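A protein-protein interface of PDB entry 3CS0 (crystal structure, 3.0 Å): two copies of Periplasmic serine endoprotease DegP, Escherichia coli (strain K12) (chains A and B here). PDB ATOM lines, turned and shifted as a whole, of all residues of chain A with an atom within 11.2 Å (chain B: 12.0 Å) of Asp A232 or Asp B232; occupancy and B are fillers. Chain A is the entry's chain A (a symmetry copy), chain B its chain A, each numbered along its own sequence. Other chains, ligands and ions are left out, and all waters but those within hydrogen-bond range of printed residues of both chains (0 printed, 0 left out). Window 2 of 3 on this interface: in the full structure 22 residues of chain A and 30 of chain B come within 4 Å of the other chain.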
ATOM      1  N   PHE A 171      21.450  -5.513  12.002  1.00  0.00           N
ATOM      2  CA  PHE A 171      22.271  -4.289  12.010  1.00  0.00           C
ATOM      3  C   PHE A 171      23.377  -4.231  10.940  1.00  0.00           C
ATOM      4  O   PHE A 171      24.485  -3.780  11.213  1.00  0.00           O
ATOM      5  CB  PHE A 171      22.930  -4.090  13.370  1.00  0.00           C
ATOM      6  CG  PHE A 171      22.026  -4.335  14.527  1.00  0.00           C
ATOM      7  CD1 PHE A 171      21.910  -5.618  15.071  1.00  0.00           C
ATOM      8  CD2 PHE A 171      21.314  -3.288  15.104  1.00  0.00           C
ATOM      9  CE1 PHE A 171      21.091  -5.862  16.191  1.00  0.00           C
ATOM     10  CE2 PHE A 171      20.492  -3.502  16.218  1.00  0.00           C
ATOM     11  CZ  PHE A 171      20.377  -4.798  16.771  1.00  0.00           C
ATOM     12  N   ILE A 205      16.358 -12.629  16.676  1.00  0.00           N
ATOM     13  CA  ILE A 205      15.968 -11.812  15.546  1.00  0.00           C
ATOM     14  C   ILE A 205      16.014 -10.346  15.961  1.00  0.00           C
ATOM     15  O   ILE A 205      15.393  -9.954  16.955  1.00  0.00           O
ATOM     16  CB  ILE A 205      14.543 -12.109  15.100  1.00  0.00           C
ATOM     17  CG1 ILE A 205      14.477 -13.429  14.371  1.00  0.00           C
ATOM     18  CG2 ILE A 205      14.075 -11.045  14.130  1.00  0.00           C
ATOM     19  CD1 ILE A 205      13.073 -13.650  13.853  1.00  0.00           C
ATOM     20  N   ASN A 206      16.741  -9.542  15.193  1.00  0.00           N
ATOM     21  CA  ASN A 206      16.854  -8.116  15.459  1.00  0.00           C
ATOM     22  C   ASN A 206      16.694  -7.323  14.175  1.00  0.00           C
ATOM     23  O   ASN A 206      16.511  -7.909  13.106  1.00  0.00           O
ATOM     24  CB  ASN A 206      18.199  -7.814  16.106  1.00  0.00           C
ATOM     25  CG  ASN A 206      18.348  -8.495  17.442  1.00  0.00           C
ATOM     26  OD1 ASN A 206      17.824  -8.019  18.454  1.00  0.00           O
ATOM     27  ND2 ASN A 206      19.042  -9.632  17.456  1.00  0.00           N
ATOM     28  N   ARG A 207      16.746  -5.993  14.285  1.00  0.00           N
ATOM     29  CA  ARG A 207      16.595  -5.117  13.131  1.00  0.00           C
ATOM     30  C   ARG A 207      17.652  -5.475  12.116  1.00  0.00           C
ATOM     31  O   ARG A 207      18.843  -5.548  12.442  1.00  0.00           O
ATOM     32  CB  ARG A 207      16.729  -3.649  13.531  1.00  0.00           C
ATOM     33  CG  ARG A 207      15.473  -3.026  14.143  1.00  0.00           C
ATOM     34  CD  ARG A 207      15.870  -1.831  15.004  1.00  0.00           C
ATOM     35  NE  ARG A 207      14.747  -1.091  15.591  1.00  0.00           N
ATOM     36  CZ  ARG A 207      13.771  -1.615  16.336  1.00  0.00           C
ATOM     37  NH1 ARG A 207      13.735  -2.915  16.610  1.00  0.00           N
ATOM     38  NH2 ARG A 207      12.842  -0.816  16.849  1.00  0.00           N
ATOM     39  N   ILE A 228       9.234  -8.506  15.814  1.00  0.00           N
ATOM     40  CA  ILE A 228       9.557  -9.037  17.135  1.00  0.00           C
ATOM     41  C   ILE A 228       8.925  -8.317  18.307  1.00  0.00           C
ATOM     42  O   ILE A 228       9.004  -7.129  18.376  1.00  0.00           O
ATOM     43  CB  ILE A 228      11.056  -8.980  17.387  1.00  0.00           C
ATOM     44  CG1 ILE A 228      11.500  -7.523  17.377  1.00  0.00           C
ATOM     45  CG2 ILE A 228      11.804  -9.762  16.324  1.00  0.00           C
ATOM     46  CD1 ILE A 228      12.849  -7.310  17.970  1.00  0.00           C
ATOM     47  N   LEU A 229       8.299  -9.018  19.240  1.00  0.00           N
ATOM     48  CA  LEU A 229       7.783  -8.300  20.395  1.00  0.00           C
ATOM     49  C   LEU A 229       9.086  -7.889  21.058  1.00  0.00           C
ATOM     50  O   LEU A 229       9.997  -8.705  21.171  1.00  0.00           O
ATOM     51  CB  LEU A 229       7.003  -9.204  21.342  1.00  0.00           C
ATOM     52  CG  LEU A 229       6.333  -8.302  22.377  1.00  0.00           C
ATOM     53  CD1 LEU A 229       5.241  -7.532  21.657  1.00  0.00           C
ATOM     54  CD2 LEU A 229       5.755  -9.094  23.537  1.00  0.00           C
ATOM     55  N   ALA A 230       9.207  -6.642  21.487  1.00  0.00           N
ATOM     56  CA  ALA A 230      10.470  -6.244  22.066  1.00  0.00           C
ATOM     57  C   ALA A 230      10.568  -4.811  22.544  1.00  0.00           C
ATOM     58  O   ALA A 230      10.662  -3.884  21.742  1.00  0.00           O
ATOM     59  CB  ALA A 230      11.574  -6.499  21.055  1.00  0.00           C
ATOM     60  N   PRO A 231      10.549  -4.607  23.865  1.00  0.00           N
ATOM     61  CA  PRO A 231      10.664  -3.241  24.373  1.00  0.00           C
ATOM     62  C   PRO A 231      12.148  -2.857  24.233  1.00  0.00           C
ATOM     63  O   PRO A 231      13.038  -3.677  24.508  1.00  0.00           O
ATOM     64  CB  PRO A 231      10.240  -3.387  25.828  1.00  0.00           C
ATOM     65  CG  PRO A 231      10.761  -4.761  26.183  1.00  0.00           C
ATOM     66  CD  PRO A 231      10.343  -5.565  24.966  1.00  0.00           C
ATOM     67  N   ASP A 232      12.416  -1.637  23.778  1.00  0.00           N
ATOM     68  CA  ASP A 232      13.795  -1.177  23.623  1.00  0.00           C
ATOM     69  C   ASP A 232      14.529  -1.911  22.502  1.00  0.00           C
ATOM     70  O   ASP A 232      15.601  -2.474  22.715  1.00  0.00           O
ATOM     71  CB  ASP A 232      14.545  -1.350  24.957  1.00  0.00           C
ATOM     72  CG  ASP A 232      15.963  -0.770  24.932  1.00  0.00           C
ATOM     73  OD1 ASP A 232      16.136   0.414  24.547  1.00  0.00           O
ATOM     74  OD2 ASP A 232      16.904  -1.504  25.318  1.00  0.00           O
ATOM     75  N   GLY A 233      13.937  -1.901  21.313  1.00  0.00           N
ATOM     76  CA  GLY A 233      14.529  -2.542  20.144  1.00  0.00           C
ATOM     77  C   GLY A 233      15.678  -3.522  20.355  1.00  0.00           C
ATOM     78  O   GLY A 233      16.799  -3.320  19.881  1.00  0.00           O
ATOM     79  N   GLY A 234      15.395  -4.595  21.076  1.00  0.00           N
ATOM     80  CA  GLY A 234      16.405  -5.595  21.328  1.00  0.00           C
ATOM     81  C   GLY A 234      15.702  -6.918  21.466  1.00  0.00           C
ATOM     82  O   GLY A 234      14.743  -7.018  22.223  1.00  0.00           O
ATOM     83  N   ASN A 235      16.154  -7.925  20.733  1.00  0.00           N
ATOM     84  CA  ASN A 235      15.532  -9.236  20.809  1.00  0.00           C
ATOM     85  C   ASN A 235      15.408  -9.721  22.260  1.00  0.00           C
ATOM     86  O   ASN A 235      16.309  -9.547  23.063  1.00  0.00           O
ATOM     87  CB  ASN A 235      16.330 -10.243  19.999  1.00  0.00           C
ATOM     88  CG  ASN A 235      15.696 -11.594  20.009  1.00  0.00           C
ATOM     89  OD1 ASN A 235      14.995 -11.973  19.062  1.00  0.00           O
ATOM     90  ND2 ASN A 235      15.900 -12.332  21.101  1.00  0.00           N
ATOM     91  N   ILE A 236      14.294 -10.359  22.579  1.00  0.00           N
ATOM     92  CA  ILE A 236      14.021 -10.819  23.934  1.00  0.00           C
ATOM     93  C   ILE A 236      13.617 -12.310  23.967  1.00  0.00           C
ATOM     94  O   ILE A 236      13.285 -12.866  25.015  1.00  0.00           O
ATOM     95  CB  ILE A 236      12.904  -9.901  24.523  1.00  0.00           C
ATOM     96  CG1 ILE A 236      13.474  -9.060  25.629  1.00  0.00           C
ATOM     97  CG2 ILE A 236      11.700 -10.676  25.044  1.00  0.00           C
ATOM     98  CD1 ILE A 236      12.440  -8.051  26.091  1.00  0.00           C
ATOM     99  N   GLY A 237      13.641 -12.964  22.814  1.00  0.00           N
ATOM    100  CA  GLY A 237      13.259 -14.359  22.795  1.00  0.00           C
ATOM    101  C   GLY A 237      11.931 -14.562  22.099  1.00  0.00           C
ATOM    102  O   GLY A 237      11.457 -15.697  21.994  1.00  0.00           O
ATOM    103  N   PHE B 171       3.840 -11.993  28.226  1.00  0.00           N
ATOM    104  CA  PHE B 171       2.972 -10.884  27.795  1.00  0.00           C
ATOM    105  C   PHE B 171       1.583 -11.299  27.276  1.00  0.00           C
ATOM    106  O   PHE B 171       1.091 -10.744  26.298  1.00  0.00           O
ATOM    107  CB  PHE B 171       3.647 -10.059  26.706  1.00  0.00           C
ATOM    108  CG  PHE B 171       5.082  -9.764  26.967  1.00  0.00           C
ATOM    109  CD1 PHE B 171       6.074 -10.651  26.537  1.00  0.00           C
ATOM    110  CD2 PHE B 171       5.458  -8.587  27.608  1.00  0.00           C
ATOM    111  CE1 PHE B 171       7.439 -10.369  26.738  1.00  0.00           C
ATOM    112  CE2 PHE B 171       6.808  -8.283  27.822  1.00  0.00           C
ATOM    113  CZ  PHE B 171       7.812  -9.177  27.384  1.00  0.00           C
ATOM    114  N   ILE B 205      12.756 -16.262  29.071  1.00  0.00           N
ATOM    115  CA  ILE B 205      11.729 -16.072  30.075  1.00  0.00           C
ATOM    116  C   ILE B 205      11.451 -14.580  30.218  1.00  0.00           C
ATOM    117  O   ILE B 205      12.372 -13.789  30.450  1.00  0.00           O
ATOM    118  CB  ILE B 205      12.174 -16.579  31.440  1.00  0.00           C
ATOM    119  CG1 ILE B 205      12.157 -18.088  31.479  1.00  0.00           C
ATOM    120  CG2 ILE B 205      11.213 -16.099  32.506  1.00  0.00           C
ATOM    121  CD1 ILE B 205      12.505 -18.561  32.873  1.00  0.00           C
ATOM    122  N   ASN B 206      10.184 -14.206  30.087  1.00  0.00           N
ATOM    123  CA  ASN B 206       9.773 -12.816  30.222  1.00  0.00           C
ATOM    124  C   ASN B 206       8.526 -12.713  31.081  1.00  0.00           C
ATOM    125  O   ASN B 206       8.006 -13.732  31.539  1.00  0.00           O
ATOM    126  CB  ASN B 206       9.523 -12.214  28.846  1.00  0.00           C
ATOM    127  CG  ASN B 206      10.770 -12.193  28.003  1.00  0.00           C
ATOM    128  OD1 ASN B 206      11.625 -11.316  28.163  1.00  0.00           O
ATOM    129  ND2 ASN B 206      10.903 -13.175  27.113  1.00  0.00           N
ATOM    130  N   ARG B 207       8.060 -11.483  31.310  1.00  0.00           N
ATOM    131  CA  ARG B 207       6.878 -11.246  32.128  1.00  0.00           C
ATOM    132  C   ARG B 207       5.720 -12.006  31.528  1.00  0.00           C
ATOM    133  O   ARG B 207       5.439 -11.888  30.329  1.00  0.00           O
ATOM    134  CB  ARG B 207       6.545  -9.757  32.200  1.00  0.00           C
ATOM    135  CG  ARG B 207       7.375  -8.955  33.203  1.00  0.00           C
ATOM    136  CD  ARG B 207       7.388  -7.486  32.788  1.00  0.00           C
ATOM    137  NE  ARG B 207       8.089  -6.589  33.714  1.00  0.00           N
ATOM    138  CZ  ARG B 207       9.346  -6.732  34.139  1.00  0.00           C
ATOM    139  NH1 ARG B 207      10.094  -7.758  33.745  1.00  0.00           N
ATOM    140  NH2 ARG B 207       9.873  -5.811  34.938  1.00  0.00           N
ATOM    141  N   ILE B 228      13.828 -13.196  36.684  1.00  0.00           N
ATOM    142  CA  ILE B 228      14.922 -13.046  35.730  1.00  0.00           C
ATOM    143  C   ILE B 228      15.858 -11.882  35.978  1.00  0.00           C
ATOM    144  O   ILE B 228      15.402 -10.796  36.166  1.00  0.00           O
ATOM    145  CB  ILE B 228      14.385 -12.839  34.322  1.00  0.00           C
ATOM    146  CG1 ILE B 228      13.588 -11.542  34.286  1.00  0.00           C
ATOM    147  CG2 ILE B 228      13.505 -14.006  33.912  1.00  0.00           C
ATOM    148  CD1 ILE B 228      13.328 -11.044  32.908  1.00  0.00           C
ATOM    149  N   LEU B 229      17.165 -12.087  35.977  1.00  0.00           N
ATOM    150  CA  LEU B 229      18.032 -10.929  36.130  1.00  0.00           C
ATOM    151  C   LEU B 229      17.770 -10.223  34.810  1.00  0.00           C
ATOM    152  O   LEU B 229      17.750 -10.870  33.767  1.00  0.00           O
ATOM    153  CB  LEU B 229      19.506 -11.310  36.209  1.00  0.00           C
ATOM    154  CG  LEU B 229      20.279 -10.050  36.591  1.00  0.00           C
ATOM    155  CD1 LEU B 229      19.927  -9.730  38.032  1.00  0.00           C
ATOM    156  CD2 LEU B 229      21.779 -10.228  36.432  1.00  0.00           C
ATOM    157  N   ALA B 230      17.555  -8.917  34.828  1.00  0.00           N
ATOM    158  CA  ALA B 230      17.252  -8.262  33.576  1.00  0.00           C
ATOM    159  C   ALA B 230      17.012  -6.769  33.639  1.00  0.00           C
ATOM    160  O   ALA B 230      15.970  -6.318  34.109  1.00  0.00           O
ATOM    161  CB  ALA B 230      16.034  -8.928  32.959  1.00  0.00           C
ATOM    162  N   PRO B 231      17.977  -5.976  33.162  1.00  0.00           N
ATOM    163  CA  PRO B 231      17.779  -4.529  33.182  1.00  0.00           C
ATOM    164  C   PRO B 231      16.811  -4.214  32.027  1.00  0.00           C
ATOM    165  O   PRO B 231      16.930  -4.790  30.933  1.00  0.00           O
ATOM    166  CB  PRO B 231      19.181  -3.995  32.922  1.00  0.00           C
ATOM    167  CG  PRO B 231      19.757  -5.033  31.988  1.00  0.00           C
ATOM    168  CD  PRO B 231      19.320  -6.320  32.661  1.00  0.00           C
ATOM    169  N   ASP B 232      15.842  -3.338  32.271  1.00  0.00           N
ATOM    170  CA  ASP B 232      14.883  -2.966  31.233  1.00  0.00           C
ATOM    171  C   ASP B 232      13.945  -4.117  30.871  1.00  0.00           C
ATOM    172  O   ASP B 232      13.826  -4.488  29.705  1.00  0.00           O
ATOM    173  CB  ASP B 232      15.642  -2.481  29.985  1.00  0.00           C
ATOM    174  CG  ASP B 232      14.719  -1.942  28.887  1.00  0.00           C
ATOM    175  OD1 ASP B 232      13.865  -1.067  29.178  1.00  0.00           O
ATOM    176  OD2 ASP B 232      14.866  -2.389  27.724  1.00  0.00           O
ATOM    177  N   GLY B 233      13.288  -4.674  31.881  1.00  0.00           N
ATOM    178  CA  GLY B 233      12.344  -5.769  31.686  1.00  0.00           C
ATOM    179  C   GLY B 233      12.353  -6.508  30.353  1.00  0.00           C
ATOM    180  O   GLY B 233      11.367  -6.520  29.611  1.00  0.00           O
ATOM    181  N   GLY B 234      13.480  -7.132  30.048  1.00  0.00           N
ATOM    182  CA  GLY B 234      13.594  -7.875  28.815  1.00  0.00           C
ATOM    183  C   GLY B 234      14.562  -9.001  29.058  1.00  0.00           C
ATOM    184  O   GLY B 234      15.651  -8.764  29.567  1.00  0.00           O
ATOM    185  N   ASN B 235      14.171 -10.220  28.719  1.00  0.00           N
ATOM    186  CA  ASN B 235      15.047 -11.363  28.919  1.00  0.00           C
ATOM    187  C   ASN B 235      16.438 -11.123  28.316  1.00  0.00           C
ATOM    188  O   ASN B 235      16.571 -10.573  27.235  1.00  0.00           O
ATOM    189  CB  ASN B 235      14.432 -12.609  28.307  1.00  0.00           C
ATOM    190  CG  ASN B 235      15.277 -13.818  28.535  1.00  0.00           C
ATOM    191  OD1 ASN B 235      15.017 -14.611  29.449  1.00  0.00           O
ATOM    192  ND2 ASN B 235      16.330 -13.959  27.730  1.00  0.00           N
ATOM    193  N   ILE B 236      17.471 -11.569  29.011  1.00  0.00           N
ATOM    194  CA  ILE B 236      18.847 -11.356  28.583  1.00  0.00           C
ATOM    195  C   ILE B 236      19.657 -12.671  28.567  1.00  0.00           C
ATOM    196  O   ILE B 236      20.858 -12.686  28.294  1.00  0.00           O
ATOM    197  CB  ILE B 236      19.476 -10.299  29.545  1.00  0.00           C
ATOM    198  CG1 ILE B 236      19.740  -9.026  28.793  1.00  0.00           C
ATOM    199  CG2 ILE B 236      20.764 -10.775  30.204  1.00  0.00           C
ATOM    200  CD1 ILE B 236      20.193  -7.945  29.756  1.00  0.00           C
ATOM    201  N   GLY B 237      18.999 -13.785  28.861  1.00  0.00           N
ATOM    202  CA  GLY B 237      19.720 -15.039  28.868  1.00  0.00           C
ATOM    203  C   GLY B 237      19.885 -15.576  30.273  1.00  0.00           C
ATOM    204  O   GLY B 237      20.478 -16.642  30.460  1.00  0.00           O
ATOM    205  N   ILE B 238      19.348 -14.859  31.262  1.00  0.00           N
ATOM    206  CA  ILE B 238      19.467 -15.288  32.649  1.00  0.00           C
ATOM    207  C   ILE B 238      18.112 -15.397  33.368  1.00  0.00           C
ATOM    208  O   ILE B 238      17.543 -14.389  33.781  1.00  0.00           O
ATOM    209  CB  ILE B 238      20.354 -14.305  33.421  1.00  0.00           C
ATOM    210  CG1 ILE B 238      21.710 -14.170  32.738  1.00  0.00           C
ATOM    211  CG2 ILE B 238      20.539 -14.768  34.838  1.00  0.00           C
ATOM    212  CD1 ILE B 238      22.656 -13.218  33.488  1.00  0.00           C
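Ile A205 touches none of the printed residues of chain B. No residue of chain B comes within 4 Å of Ala A230. Pro A231 touches just these residues of chain B: Asp B232 (3.9 Å) and Gly B233 (3.9 Å). No residue of chain B comes within 4 Å of Gly A233. No residue of chain B comes within 4 Å of Gly A234. Of the printed residues of chain A, Asn B206 touches Ile A236. No residue of chain A comes within 4 Å of Ala B230. Pro B231 touches none of the printed residues of chain A. Of chain A, only Pro A231 (3.9 Å) and Asp A232 (3.0 Å) come within 4 Å of Asp B232. Of the printed residues of chain A, Gly B233 touches Pro A231 (3.9 Å) and Ile A236 (3.99 Å). Gly B234 touches just one residue of chain A: Ile A236 (3.0 Å). The nearest residue of chain B that does not touch Asp A232 is Pro B231 (6.5 Å). The nearest residue of chain A that does not touch Asp B232 is Ile A236 (5.3 Å).
Pro A231 touches Asp B232, but with the chains exchanged Asp A232 does not touch Pro B231 (6.5 Å). Asp B232 touches its own counterpart, Asp A232. Ile A236 touches Asn B206, but with the chains exchanged Asn A206 does not touch Ile B236 (10.6 Å). Ile A236 touches Gly B234, but with the chains exchanged Gly A234 does not touch Ile B236 (8.5 Å). 14 positions are printed for both chains.
N of Phe B171 sits at hydrogen-bond distance from O of Arg B207, 2.6 Å away. ND2 of Asn B235 sits close to N of Gly B237 (2.9 Å). The side-chain amide oxygen (OD1) of Asn B206 sits at hydrogen-bond distance from the backbone NH (N) of Asn B235 (2.8 Å). The backbone NH (N) of Ile B205 lies within hydrogen-bond range of the side-chain amide oxygen (OD1) of Asn B235 (2.8 Å).
Among the printed residues, merely in contact across the chains: Ile A236 with Gly B234 (3.0 Å), Ile A236 with Asn B235 (3.4 Å), Leu A229 with Phe B171 (3.4 Å), Pro A231 with Gly B233 (3.9 Å), Pro A231 with Asp B232 (3.9 Å) and Ile A236 with Gly B233 (3.99 Å).
The side-chain carboxylate of Asp A232 sits close to the side-chain carboxylate of Asp B232. ND2 of Asn B206 sits at hydrogen-bond distance from O of Ile A236, at 3.2 Å.
Among the printed residues, 8 pairs touch across the chains.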
